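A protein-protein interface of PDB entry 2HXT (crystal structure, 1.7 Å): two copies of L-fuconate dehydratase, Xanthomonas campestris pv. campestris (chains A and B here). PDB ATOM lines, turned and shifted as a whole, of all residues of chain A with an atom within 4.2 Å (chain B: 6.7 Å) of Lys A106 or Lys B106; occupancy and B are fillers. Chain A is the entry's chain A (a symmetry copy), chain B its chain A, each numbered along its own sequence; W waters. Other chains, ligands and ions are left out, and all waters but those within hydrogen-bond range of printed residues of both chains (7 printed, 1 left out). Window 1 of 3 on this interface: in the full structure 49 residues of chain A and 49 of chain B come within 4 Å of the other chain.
Printed residues of chain B within 4 Å of Lys A106: Lys B106, Asp B280 and Gln B304.
Of the printed residues of chain B, His A302 touches Pro B104 (3.5 Å).
Printed residues of chain A within 4 Å of Pro B104: His A302 (3.5 Å).
Of the printed residues of chain A, Lys B106 touches Lys A106 (3.99 Å), Asp A280 (2.7 Å) and Gln A304 (2.8 Å).
Printed residues of chain A within 4 Å of Asp B280: Lys A106 (2.7 Å) and Gln A304 (2.9 Å).
Of the printed residues of chain A, Gln B304 touches Lys A106, Asp A280 and Gln A304.
The nearest printed residue of chain B that does not touch Lys A106 is His B302 (4.02 Å).
Water W4 lies within hydrogen-bond range of O of His A302 (2.6 Å), O of Gly B103 (2.7 Å) and NZ of Lys B106 (2.8 Å).
Water W6 lies within hydrogen-bond range of the backbone carbonyl oxygen (O) of His B302 (2.6 Å), the backbone carbonyl oxygen (O) of Gly A103 (2.7 Å) and the side-chain amino group (NZ) of Lys A106 (2.8 Å).
Water W1 lies within hydrogen-bond range of the side-chain carboxylate (OD2) of Asp A280 and the backbone carbonyl oxygen (O) of Pro B104.
Water W2 lies within hydrogen-bond range of O of Lys A106, N of Val B108 and N of Val A108.
Water W3 lies within hydrogen-bond range of OD1 of Asp B280 (3.1 Å), NE2 of Gln B304 (3.2 Å) and OE1 of Gln A304 (3.4 Å).
Water W5 lies within hydrogen-bond range of OD1 of Asp A280 (3.1 Å), NE2 of Gln A304 (3.2 Å) and OE1 of Gln B304 (3.4 Å).
His B302 touches Pro A104 (CD2 to CG, 3.5 Å).
Lys B106 touches Lys A106.
O of Leu B102 touches CA of Gly A107, 3.5 Å away.
Val A108 touches Val B108 (CB to CB, 3.9 Å).
His A302 touches Pro B104.
Hydrophobic or aromatic side chains of chain B that line the printed part of chain A: Leu B102, Pro B104, Val B108 and His B302.
Along chain B the printed residues that touch a printed residue of chain A span positions 102 to 327.
Lys B106 touches its own counterpart, Lys A106.
Lys A106 touches Asp B280, and with the chains exchanged Asp A280 touches Lys B106.
Asp A280 touches Gln B304, and with the chains exchanged Gln A304 touches Asp B280.
Gln A304 touches its own counterpart, Gln B304.
Of the 15 pairs that touch across the chains among the printed residues, 11 have their exchanged pair printed and touching as well.
The guanidinium group of Arg B327 sits close to a ring nitrogen (ND1) of His B302 (3.4 Å).
The backbone carbonyl oxygen (O) of Glu B105 is in hydrogen-bond range of the side-chain amide nitrogen (ND2) of Asn B305, 2.9 Å away.
SD of Met B111 sits close to NH2 of Arg B327, at 3.6 Å.
The side-chain carboxylate (OD1) of Asp B280 lies within hydrogen-bond range of the side-chain amide nitrogen (NE2) of Gln B304.
The side-chain amide nitrogen (NE2) of Gln A304 lies within hydrogen-bond range of the side-chain carboxylate (OD1) of Asp A280 (3.4 Å).
The side-chain amide nitrogen of Gln B304 is in hydrogen-bond range of the side-chain amide oxygen of Gln A304, 3.0 Å away.
NZ of Lys B106 sits close to NE2 of Gln A304, 2.8 Å away.
The backbone carbonyl oxygen (O) of Gly A103 is in hydrogen-bond range of the guanidinium group (NH2) of Arg B327 (2.9 Å).
NZ of Lys B106 is in salt-bridge range of OD1 of Asp A280, 2.7 Å away.
The side-chain amide oxygen of Gln B304 sits close to the side-chain carboxylate of Asp A280, 2.9 Å away.
ND2 of Asn B305 sits at hydrogen-bond distance from OD2 of Asp A280 (3.0 Å).
The side-chain amino group of Lys A106 lies within salt-bridge range of the side-chain carboxylate of Asp B280 (2.7 Å).
The backbone carbonyl oxygen (O) of Leu B102 sits at hydrogen-bond distance from the backbone NH (N) of Val A108 (3.5 Å).
OD2 of Asp B280 lies close to OE1 of Gln A304 (2.9 Å).
NE2 of Gln B304 sits close to NZ of Lys A106.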
ATOM      1  N   GLY A 103      28.289 -22.987   3.382  1.00  0.00           N
ATOM      2  CA  GLY A 103      28.157 -22.799   1.949  1.00  0.00           C
ATOM      3  C   GLY A 103      29.418 -22.121   1.448  1.00  0.00           C
ATOM      4  O   GLY A 103      30.440 -22.785   1.270  1.00  0.00           O
ATOM      5  N   PRO A 104      29.387 -20.798   1.218  1.00  0.00           N
ATOM      6  CA  PRO A 104      28.218 -19.926   1.393  1.00  0.00           C
ATOM      7  C   PRO A 104      27.326 -19.952   0.157  1.00  0.00           C
ATOM      8  O   PRO A 104      27.816 -20.062  -0.963  1.00  0.00           O
ATOM      9  CB  PRO A 104      28.832 -18.533   1.593  1.00  0.00           C
ATOM     10  CG  PRO A 104      30.313 -18.789   1.843  1.00  0.00           C
ATOM     11  CD  PRO A 104      30.601 -19.996   1.004  1.00  0.00           C
ATOM     12  N   GLU A 105      26.020 -19.846   0.367  1.00  0.00           N
ATOM     13  CA  GLU A 105      25.065 -19.822  -0.732  1.00  0.00           C
ATOM     14  C   GLU A 105      25.266 -20.929  -1.766  1.00  0.00           C
ATOM     15  O   GLU A 105      25.295 -20.677  -2.974  1.00  0.00           O
ATOM     16  CB  GLU A 105      25.100 -18.447  -1.409  1.00  0.00           C
ATOM     17  CG  GLU A 105      24.951 -17.299  -0.416  1.00  0.00           C
ATOM     18  CD  GLU A 105      24.884 -15.934  -1.077  1.00  0.00           C
ATOM     19  OE1 GLU A 105      25.171 -14.931  -0.388  1.00  0.00           O
ATOM     20  OE2 GLU A 105      24.537 -15.859  -2.276  1.00  0.00           O
ATOM     21  N   LYS A 106      25.398 -22.158  -1.278  1.00  0.00           N
ATOM     22  CA  LYS A 106      25.561 -23.316  -2.144  1.00  0.00           C
ATOM     23  C   LYS A 106      25.332 -24.582  -1.328  1.00  0.00           C
ATOM     24  O   LYS A 106      25.409 -24.566  -0.095  1.00  0.00           O
ATOM     25  CB  LYS A 106      26.973 -23.348  -2.740  1.00  0.00           C
ATOM     26  CG  LYS A 106      28.056 -23.708  -1.729  1.00  0.00           C
ATOM     27  CD  LYS A 106      29.452 -23.503  -2.301  1.00  0.00           C
ATOM     28  CE  LYS A 106      29.764 -22.021  -2.449  1.00  0.00           C
ATOM     29  NZ  LYS A 106      31.194 -21.804  -2.811  1.00  0.00           N
ATOM     30  N   GLY A 107      25.039 -25.675  -2.026  1.00  0.00           N
ATOM     31  CA  GLY A 107      24.848 -26.952  -1.363  1.00  0.00           C
ATOM     32  C   GLY A 107      23.642 -27.106  -0.463  1.00  0.00           C
ATOM     33  O   GLY A 107      22.688 -26.331  -0.522  1.00  0.00           O
ATOM     34  N   VAL A 108      23.714 -28.127   0.385  1.00  0.00           N
ATOM     35  CA  VAL A 108      22.646 -28.471   1.316  1.00  0.00           C
ATOM     36  C   VAL A 108      22.093 -27.335   2.166  1.00  0.00           C
ATOM     37  O   VAL A 108      20.878 -27.141   2.231  1.00  0.00           O
ATOM     38  CB  VAL A 108      23.099 -29.611   2.273  1.00  0.00           C
ATOM     39  CG1 VAL A 108      22.051 -29.834   3.354  1.00  0.00           C
ATOM     40  CG2 VAL A 108      23.317 -30.898   1.490  1.00  0.00           C
ATOM     41  N   HIS A 110      22.202 -24.063   1.745  1.00  0.00           N
ATOM     42  CA  HIS A 110      21.535 -23.020   0.973  1.00  0.00           C
ATOM     43  C   HIS A 110      20.203 -23.502   0.405  1.00  0.00           C
ATOM     44  O   HIS A 110      19.234 -22.742   0.369  1.00  0.00           O
ATOM     45  CB  HIS A 110      22.436 -22.528  -0.159  1.00  0.00           C
ATOM     46  CG  HIS A 110      21.997 -21.226  -0.758  1.00  0.00           C
ATOM     47  ND1 HIS A 110      21.703 -20.117   0.008  1.00  0.00           N
ATOM     48  CD2 HIS A 110      21.847 -20.843  -2.048  1.00  0.00           C
ATOM     49  CE1 HIS A 110      21.393 -19.106  -0.786  1.00  0.00           C
ATOM     50  NE2 HIS A 110      21.474 -19.520  -2.038  1.00  0.00           N
ATOM     51  N   ASP A 280      30.040 -25.914 -12.381  1.00  0.00           N
ATOM     52  CA  ASP A 280      30.891 -24.869 -11.819  1.00  0.00           C
ATOM     53  C   ASP A 280      31.866 -24.308 -12.847  1.00  0.00           C
ATOM     54  O   ASP A 280      32.519 -23.298 -12.590  1.00  0.00           O
ATOM     55  CB  ASP A 280      31.732 -25.402 -10.657  1.00  0.00           C
ATOM     56  CG  ASP A 280      30.898 -25.966  -9.536  1.00  0.00           C
ATOM     57  OD1 ASP A 280      29.767 -25.483  -9.326  1.00  0.00           O
ATOM     58  OD2 ASP A 280      31.393 -26.884  -8.850  1.00  0.00           O
ATOM     59  N   HIS A 302      21.779 -26.791 -11.717  1.00  0.00           N
ATOM     60  CA  HIS A 302      22.650 -26.997 -10.561  1.00  0.00           C
ATOM     61  C   HIS A 302      23.460 -25.738 -10.251  1.00  0.00           C
ATOM     62  O   HIS A 302      24.295 -25.744  -9.347  1.00  0.00           O
ATOM     63  CB  HIS A 302      23.613 -28.165 -10.804  1.00  0.00           C
ATOM     64  CG  HIS A 302      23.081 -29.502 -10.387  1.00  0.00           C
ATOM     65  ND1 HIS A 302      21.735 -29.762 -10.231  1.00  0.00           N
ATOM     66  CD2 HIS A 302      23.719 -30.672 -10.146  1.00  0.00           C
ATOM     67  CE1 HIS A 302      21.568 -31.035  -9.915  1.00  0.00           C
ATOM     68  NE2 HIS A 302      22.757 -31.609  -9.857  1.00  0.00           N
ATOM     69  N   GLN A 304      24.643 -22.919  -8.471  1.00  0.00           N
ATOM     70  CA  GLN A 304      24.458 -22.631  -7.051  1.00  0.00           C
ATOM     71  C   GLN A 304      23.827 -21.321  -6.594  1.00  0.00           C
ATOM     72  O   GLN A 304      23.103 -21.306  -5.599  1.00  0.00           O
ATOM     73  CB  GLN A 304      25.789 -22.838  -6.326  1.00  0.00           C
ATOM     74  CG  GLN A 304      26.857 -21.823  -6.675  1.00  0.00           C
ATOM     75  CD  GLN A 304      28.247 -22.346  -6.391  1.00  0.00           C
ATOM     76  OE1 GLN A 304      29.087 -21.649  -5.823  1.00  0.00           O
ATOM     77  NE2 GLN A 304      28.498 -23.581  -6.793  1.00  0.00           N
ATOM     78  N   LEU B 102      23.316 -33.286  -3.906  1.00  0.00           N
ATOM     79  CA  LEU B 102      23.324 -32.341  -2.793  1.00  0.00           C
ATOM     80  C   LEU B 102      24.429 -31.297  -2.928  1.00  0.00           C
ATOM     81  O   LEU B 102      24.512 -30.359  -2.132  1.00  0.00           O
ATOM     82  CB  LEU B 102      23.476 -33.086  -1.462  1.00  0.00           C
ATOM     83  CG  LEU B 102      22.207 -33.678  -0.840  1.00  0.00           C
ATOM     84  CD1 LEU B 102      21.516 -34.619  -1.809  1.00  0.00           C
ATOM     85  CD2 LEU B 102      22.581 -34.403   0.441  1.00  0.00           C
ATOM     86  N   GLY B 103      25.268 -31.473  -3.943  1.00  0.00           N
ATOM     87  CA  GLY B 103      26.350 -30.541  -4.201  1.00  0.00           C
ATOM     88  C   GLY B 103      26.150 -29.965  -5.590  1.00  0.00           C
ATOM     89  O   GLY B 103      25.328 -29.066  -5.767  1.00  0.00           O
ATOM     90  N   PRO B 104      26.879 -30.464  -6.602  1.00  0.00           N
ATOM     91  CA  PRO B 104      27.885 -31.529  -6.488  1.00  0.00           C
ATOM     92  C   PRO B 104      29.237 -30.960  -6.069  1.00  0.00           C
ATOM     93  O   PRO B 104      29.593 -29.851  -6.456  1.00  0.00           O
ATOM     94  CB  PRO B 104      27.956 -32.114  -7.905  1.00  0.00           C
ATOM     95  CG  PRO B 104      26.739 -31.546  -8.625  1.00  0.00           C
ATOM     96  CD  PRO B 104      26.579 -30.188  -8.014  1.00  0.00           C
ATOM     97  N   GLU B 105      29.984 -31.726  -5.285  1.00  0.00           N
ATOM     98  CA  GLU B 105      31.309 -31.313  -4.844  1.00  0.00           C
ATOM     99  C   GLU B 105      31.373 -29.894  -4.281  1.00  0.00           C
ATOM    100  O   GLU B 105      32.234 -29.095  -4.658  1.00  0.00           O
ATOM    101  CB  GLU B 105      32.303 -31.473  -6.000  1.00  0.00           C
ATOM    102  CG  GLU B 105      32.251 -32.859  -6.633  1.00  0.00           C
ATOM    103  CD  GLU B 105      33.296 -33.068  -7.714  1.00  0.00           C
ATOM    104  OE1 GLU B 105      33.097 -33.968  -8.560  1.00  0.00           O
ATOM    105  OE2 GLU B 105      34.318 -32.348  -7.716  1.00  0.00           O
ATOM    106  N   LYS B 106      30.454 -29.593  -3.369  1.00  0.00           N
ATOM    107  CA  LYS B 106      30.411 -28.293  -2.719  1.00  0.00           C
ATOM    108  C   LYS B 106      29.499 -28.374  -1.502  1.00  0.00           C
ATOM    109  O   LYS B 106      28.667 -29.281  -1.391  1.00  0.00           O
ATOM    110  CB  LYS B 106      29.876 -27.227  -3.682  1.00  0.00           C
ATOM    111  CG  LYS B 106      28.383 -27.351  -3.962  1.00  0.00           C
ATOM    112  CD  LYS B 106      27.941 -26.429  -5.090  1.00  0.00           C
ATOM    113  CE  LYS B 106      28.466 -26.923  -6.429  1.00  0.00           C
ATOM    114  NZ  LYS B 106      27.874 -26.152  -7.559  1.00  0.00           N
ATOM    115  N   GLY B 107      29.669 -27.427  -0.586  1.00  0.00           N
ATOM    116  CA  GLY B 107      28.825 -27.371   0.593  1.00  0.00           C
ATOM    117  C   GLY B 107      28.956 -28.486   1.607  1.00  0.00           C
ATOM    118  O   GLY B 107      29.934 -29.233   1.624  1.00  0.00           O
ATOM    119  N   VAL B 108      27.934 -28.587   2.451  1.00  0.00           N
ATOM    120  CA  VAL B 108      27.876 -29.571   3.524  1.00  0.00           C
ATOM    121  C   VAL B 108      28.169 -31.016   3.138  1.00  0.00           C
ATOM    122  O   VAL B 108      28.987 -31.677   3.778  1.00  0.00           O
ATOM    123  CB  VAL B 108      26.490 -29.534   4.229  1.00  0.00           C
ATOM    124  CG1 VAL B 108      26.374 -30.684   5.219  1.00  0.00           C
ATOM    125  CG2 VAL B 108      26.305 -28.207   4.953  1.00  0.00           C
ATOM    126  N   MET B 109      27.510 -31.523   2.101  1.00  0.00           N
ATOM    127  CA  MET B 109      27.728 -32.918   1.736  1.00  0.00           C
ATOM    128  C   MET B 109      29.152 -33.207   1.279  1.00  0.00           C
ATOM    129  O   MET B 109      29.705 -34.256   1.602  1.00  0.00           O
ATOM    130  CB  MET B 109      26.725 -33.365   0.667  1.00  0.00           C
ATOM    131  CG  MET B 109      26.485 -34.880   0.638  1.00  0.00           C
ATOM    132  SD  MET B 109      25.720 -35.559   2.159  1.00  0.00           S
ATOM    133  CE  MET B 109      27.095 -36.479   2.854  1.00  0.00           C
ATOM    134  N   HIS B 110      29.757 -32.283   0.538  1.00  0.00           N
ATOM    135  CA  HIS B 110      31.120 -32.504   0.069  1.00  0.00           C
ATOM    136  C   HIS B 110      32.134 -32.400   1.206  1.00  0.00           C
ATOM    137  O   HIS B 110      33.099 -33.163   1.248  1.00  0.00           O
ATOM    138  CB  HIS B 110      31.477 -31.512  -1.037  1.00  0.00           C
ATOM    139  CG  HIS B 110      32.695 -31.895  -1.823  1.00  0.00           C
ATOM    140  ND1 HIS B 110      32.864 -33.152  -2.367  1.00  0.00           N
ATOM    141  CD2 HIS B 110      33.779 -31.175  -2.197  1.00  0.00           C
ATOM    142  CE1 HIS B 110      34.000 -33.188  -3.043  1.00  0.00           C
ATOM    143  NE2 HIS B 110      34.573 -32.001  -2.957  1.00  0.00           N
ATOM    144  N   MET B 111      31.929 -31.461   2.126  1.00  0.00           N
ATOM    145  CA  MET B 111      32.859 -31.339   3.245  1.00  0.00           C
ATOM    146  C   MET B 111      32.753 -32.591   4.121  1.00  0.00           C
ATOM    147  O   MET B 111      33.756 -33.062   4.654  1.00  0.00           O
ATOM    148  CB  MET B 111      32.593 -30.065   4.070  1.00  0.00           C
ATOM    149  CG  MET B 111      32.992 -28.756   3.355  1.00  0.00           C
ATOM    150  SD  MET B 111      33.174 -27.271   4.431  1.00  0.00           S
ATOM    151  CE  MET B 111      31.383 -26.885   4.767  1.00  0.00           C
ATOM    152  N   PRO B 279      33.604 -15.936  -2.844  1.00  0.00           N
ATOM    153  CA  PRO B 279      34.503 -17.046  -3.171  1.00  0.00           C
ATOM    154  C   PRO B 279      34.127 -17.752  -4.471  1.00  0.00           C
ATOM    155  O   PRO B 279      34.849 -18.634  -4.939  1.00  0.00           O
ATOM    156  CB  PRO B 279      34.383 -17.958  -1.950  1.00  0.00           C
ATOM    157  CG  PRO B 279      32.969 -17.748  -1.526  1.00  0.00           C
ATOM    158  CD  PRO B 279      32.802 -16.246  -1.646  1.00  0.00           C
ATOM    159  N   ASP B 280      32.994 -17.360  -5.049  1.00  0.00           N
ATOM    160  CA  ASP B 280      32.532 -17.944  -6.305  1.00  0.00           C
ATOM    161  C   ASP B 280      32.804 -17.034  -7.497  1.00  0.00           C
ATOM    162  O   ASP B 280      32.650 -17.455  -8.641  1.00  0.00           O
ATOM    163  CB  ASP B 280      31.023 -18.200  -6.279  1.00  0.00           C
ATOM    164  CG  ASP B 280      30.600 -19.120  -5.163  1.00  0.00           C
ATOM    165  OD1 ASP B 280      31.395 -19.999  -4.775  1.00  0.00           O
ATOM    166  OD2 ASP B 280      29.455 -18.969  -4.690  1.00  0.00           O
ATOM    167  N   HIS B 302      37.487 -20.930   0.994  1.00  0.00           N
ATOM    168  CA  HIS B 302      36.101 -21.331   0.752  1.00  0.00           C
ATOM    169  C   HIS B 302      35.919 -21.851  -0.674  1.00  0.00           C
ATOM    170  O   HIS B 302      34.803 -22.176  -1.078  1.00  0.00           O
ATOM    171  CB  HIS B 302      35.145 -20.156   0.985  1.00  0.00           C
ATOM    172  CG  HIS B 302      34.651 -20.031   2.394  1.00  0.00           C
ATOM    173  ND1 HIS B 302      35.303 -20.590   3.474  1.00  0.00           N
ATOM    174  CD2 HIS B 302      33.591 -19.358   2.903  1.00  0.00           C
ATOM    175  CE1 HIS B 302      34.666 -20.265   4.586  1.00  0.00           C
ATOM    176  NE2 HIS B 302      33.624 -19.517   4.267  1.00  0.00           N
ATOM    177  N   THR B 303      37.000 -21.924  -1.446  1.00  0.00           N
ATOM    178  CA  THR B 303      36.885 -22.422  -2.817  1.00  0.00           C
ATOM    179  C   THR B 303      36.386 -23.857  -2.725  1.00  0.00           C
ATOM    180  O   THR B 303      37.036 -24.720  -2.142  1.00  0.00           O
ATOM    181  CB  THR B 303      38.229 -22.341  -3.541  1.00  0.00           C
ATOM    182  OG1 THR B 303      38.698 -20.988  -3.482  1.00  0.00           O
ATOM    183  CG2 THR B 303      38.070 -22.745  -5.002  1.00  0.00           C
ATOM    184  N   GLN B 304      35.218 -24.100  -3.313  1.00  0.00           N
ATOM    185  CA  GLN B 304      34.550 -25.395  -3.214  1.00  0.00           C
ATOM    186  C   GLN B 304      35.218 -26.661  -3.737  1.00  0.00           C
ATOM    187  O   GLN B 304      35.051 -27.728  -3.145  1.00  0.00           O
ATOM    188  CB  GLN B 304      33.146 -25.274  -3.809  1.00  0.00           C
ATOM    189  CG  GLN B 304      33.116 -25.064  -5.308  1.00  0.00           C
ATOM    190  CD  GLN B 304      31.822 -24.427  -5.762  1.00  0.00           C
ATOM    191  OE1 GLN B 304      31.216 -24.847  -6.748  1.00  0.00           O
ATOM    192  NE2 GLN B 304      31.394 -23.401  -5.046  1.00  0.00           N
ATOM    193  N   ASN B 305      35.960 -26.567  -4.833  1.00  0.00           N
ATOM    194  CA  ASN B 305      36.606 -27.751  -5.381  1.00  0.00           C
ATOM    195  C   ASN B 305      37.698 -27.388  -6.377  1.00  0.00           C
ATOM    196  O   ASN B 305      37.931 -26.211  -6.658  1.00  0.00           O
ATOM    197  CB  ASN B 305      35.564 -28.666  -6.042  1.00  0.00           C
ATOM    198  CG  ASN B 305      34.800 -27.973  -7.149  1.00  0.00           C
ATOM    199  OD1 ASN B 305      35.395 -27.361  -8.032  1.00  0.00           O
ATOM    200  ND2 ASN B 305      33.471 -28.070  -7.113  1.00  0.00           N
ATOM    201  N   ARG B 327      37.765 -27.981   3.488  1.00  0.00           N
ATOM    202  CA  ARG B 327      36.755 -27.391   2.612  1.00  0.00           C
ATOM    203  C   ARG B 327      36.409 -28.239   1.386  1.00  0.00           C
ATOM    204  O   ARG B 327      35.263 -28.245   0.937  1.00  0.00           O
ATOM    205  CB  ARG B 327      37.216 -25.994   2.165  1.00  0.00           C
ATOM    206  CG  ARG B 327      36.331 -25.298   1.119  1.00  0.00           C
ATOM    207  CD  ARG B 327      34.893 -25.078   1.590  1.00  0.00           C
ATOM    208  NE  ARG B 327      34.804 -24.384   2.873  1.00  0.00           N
ATOM    209  CZ  ARG B 327      33.663 -23.975   3.424  1.00  0.00           C
ATOM    210  NH1 ARG B 327      33.673 -23.359   4.599  1.00  0.00           N
ATOM    211  NH2 ARG B 327      32.509 -24.165   2.796  1.00  0.00           N
HETATM  212  O   HOH W   1      29.769 -28.918  -8.945  1.00  0.00           O
HETATM  213  O   HOH W   2      25.814 -26.258   2.040  1.00  0.00           O
HETATM  214  O   HOH W   3      32.081 -21.365  -7.422  1.00  0.00           O
HETATM  215  O   HOH W   4      25.174 -26.761  -7.126  1.00  0.00           O
HETATM  216  O   HOH W   5      30.443 -22.510  -9.102  1.00  0.00           O
HETATM  217  O   HOH W   6      32.386 -22.973  -0.562  1.00  0.00           O
HETATM  218  O   HOH W   7      29.693 -18.572  -2.127  1.00  0.00           O
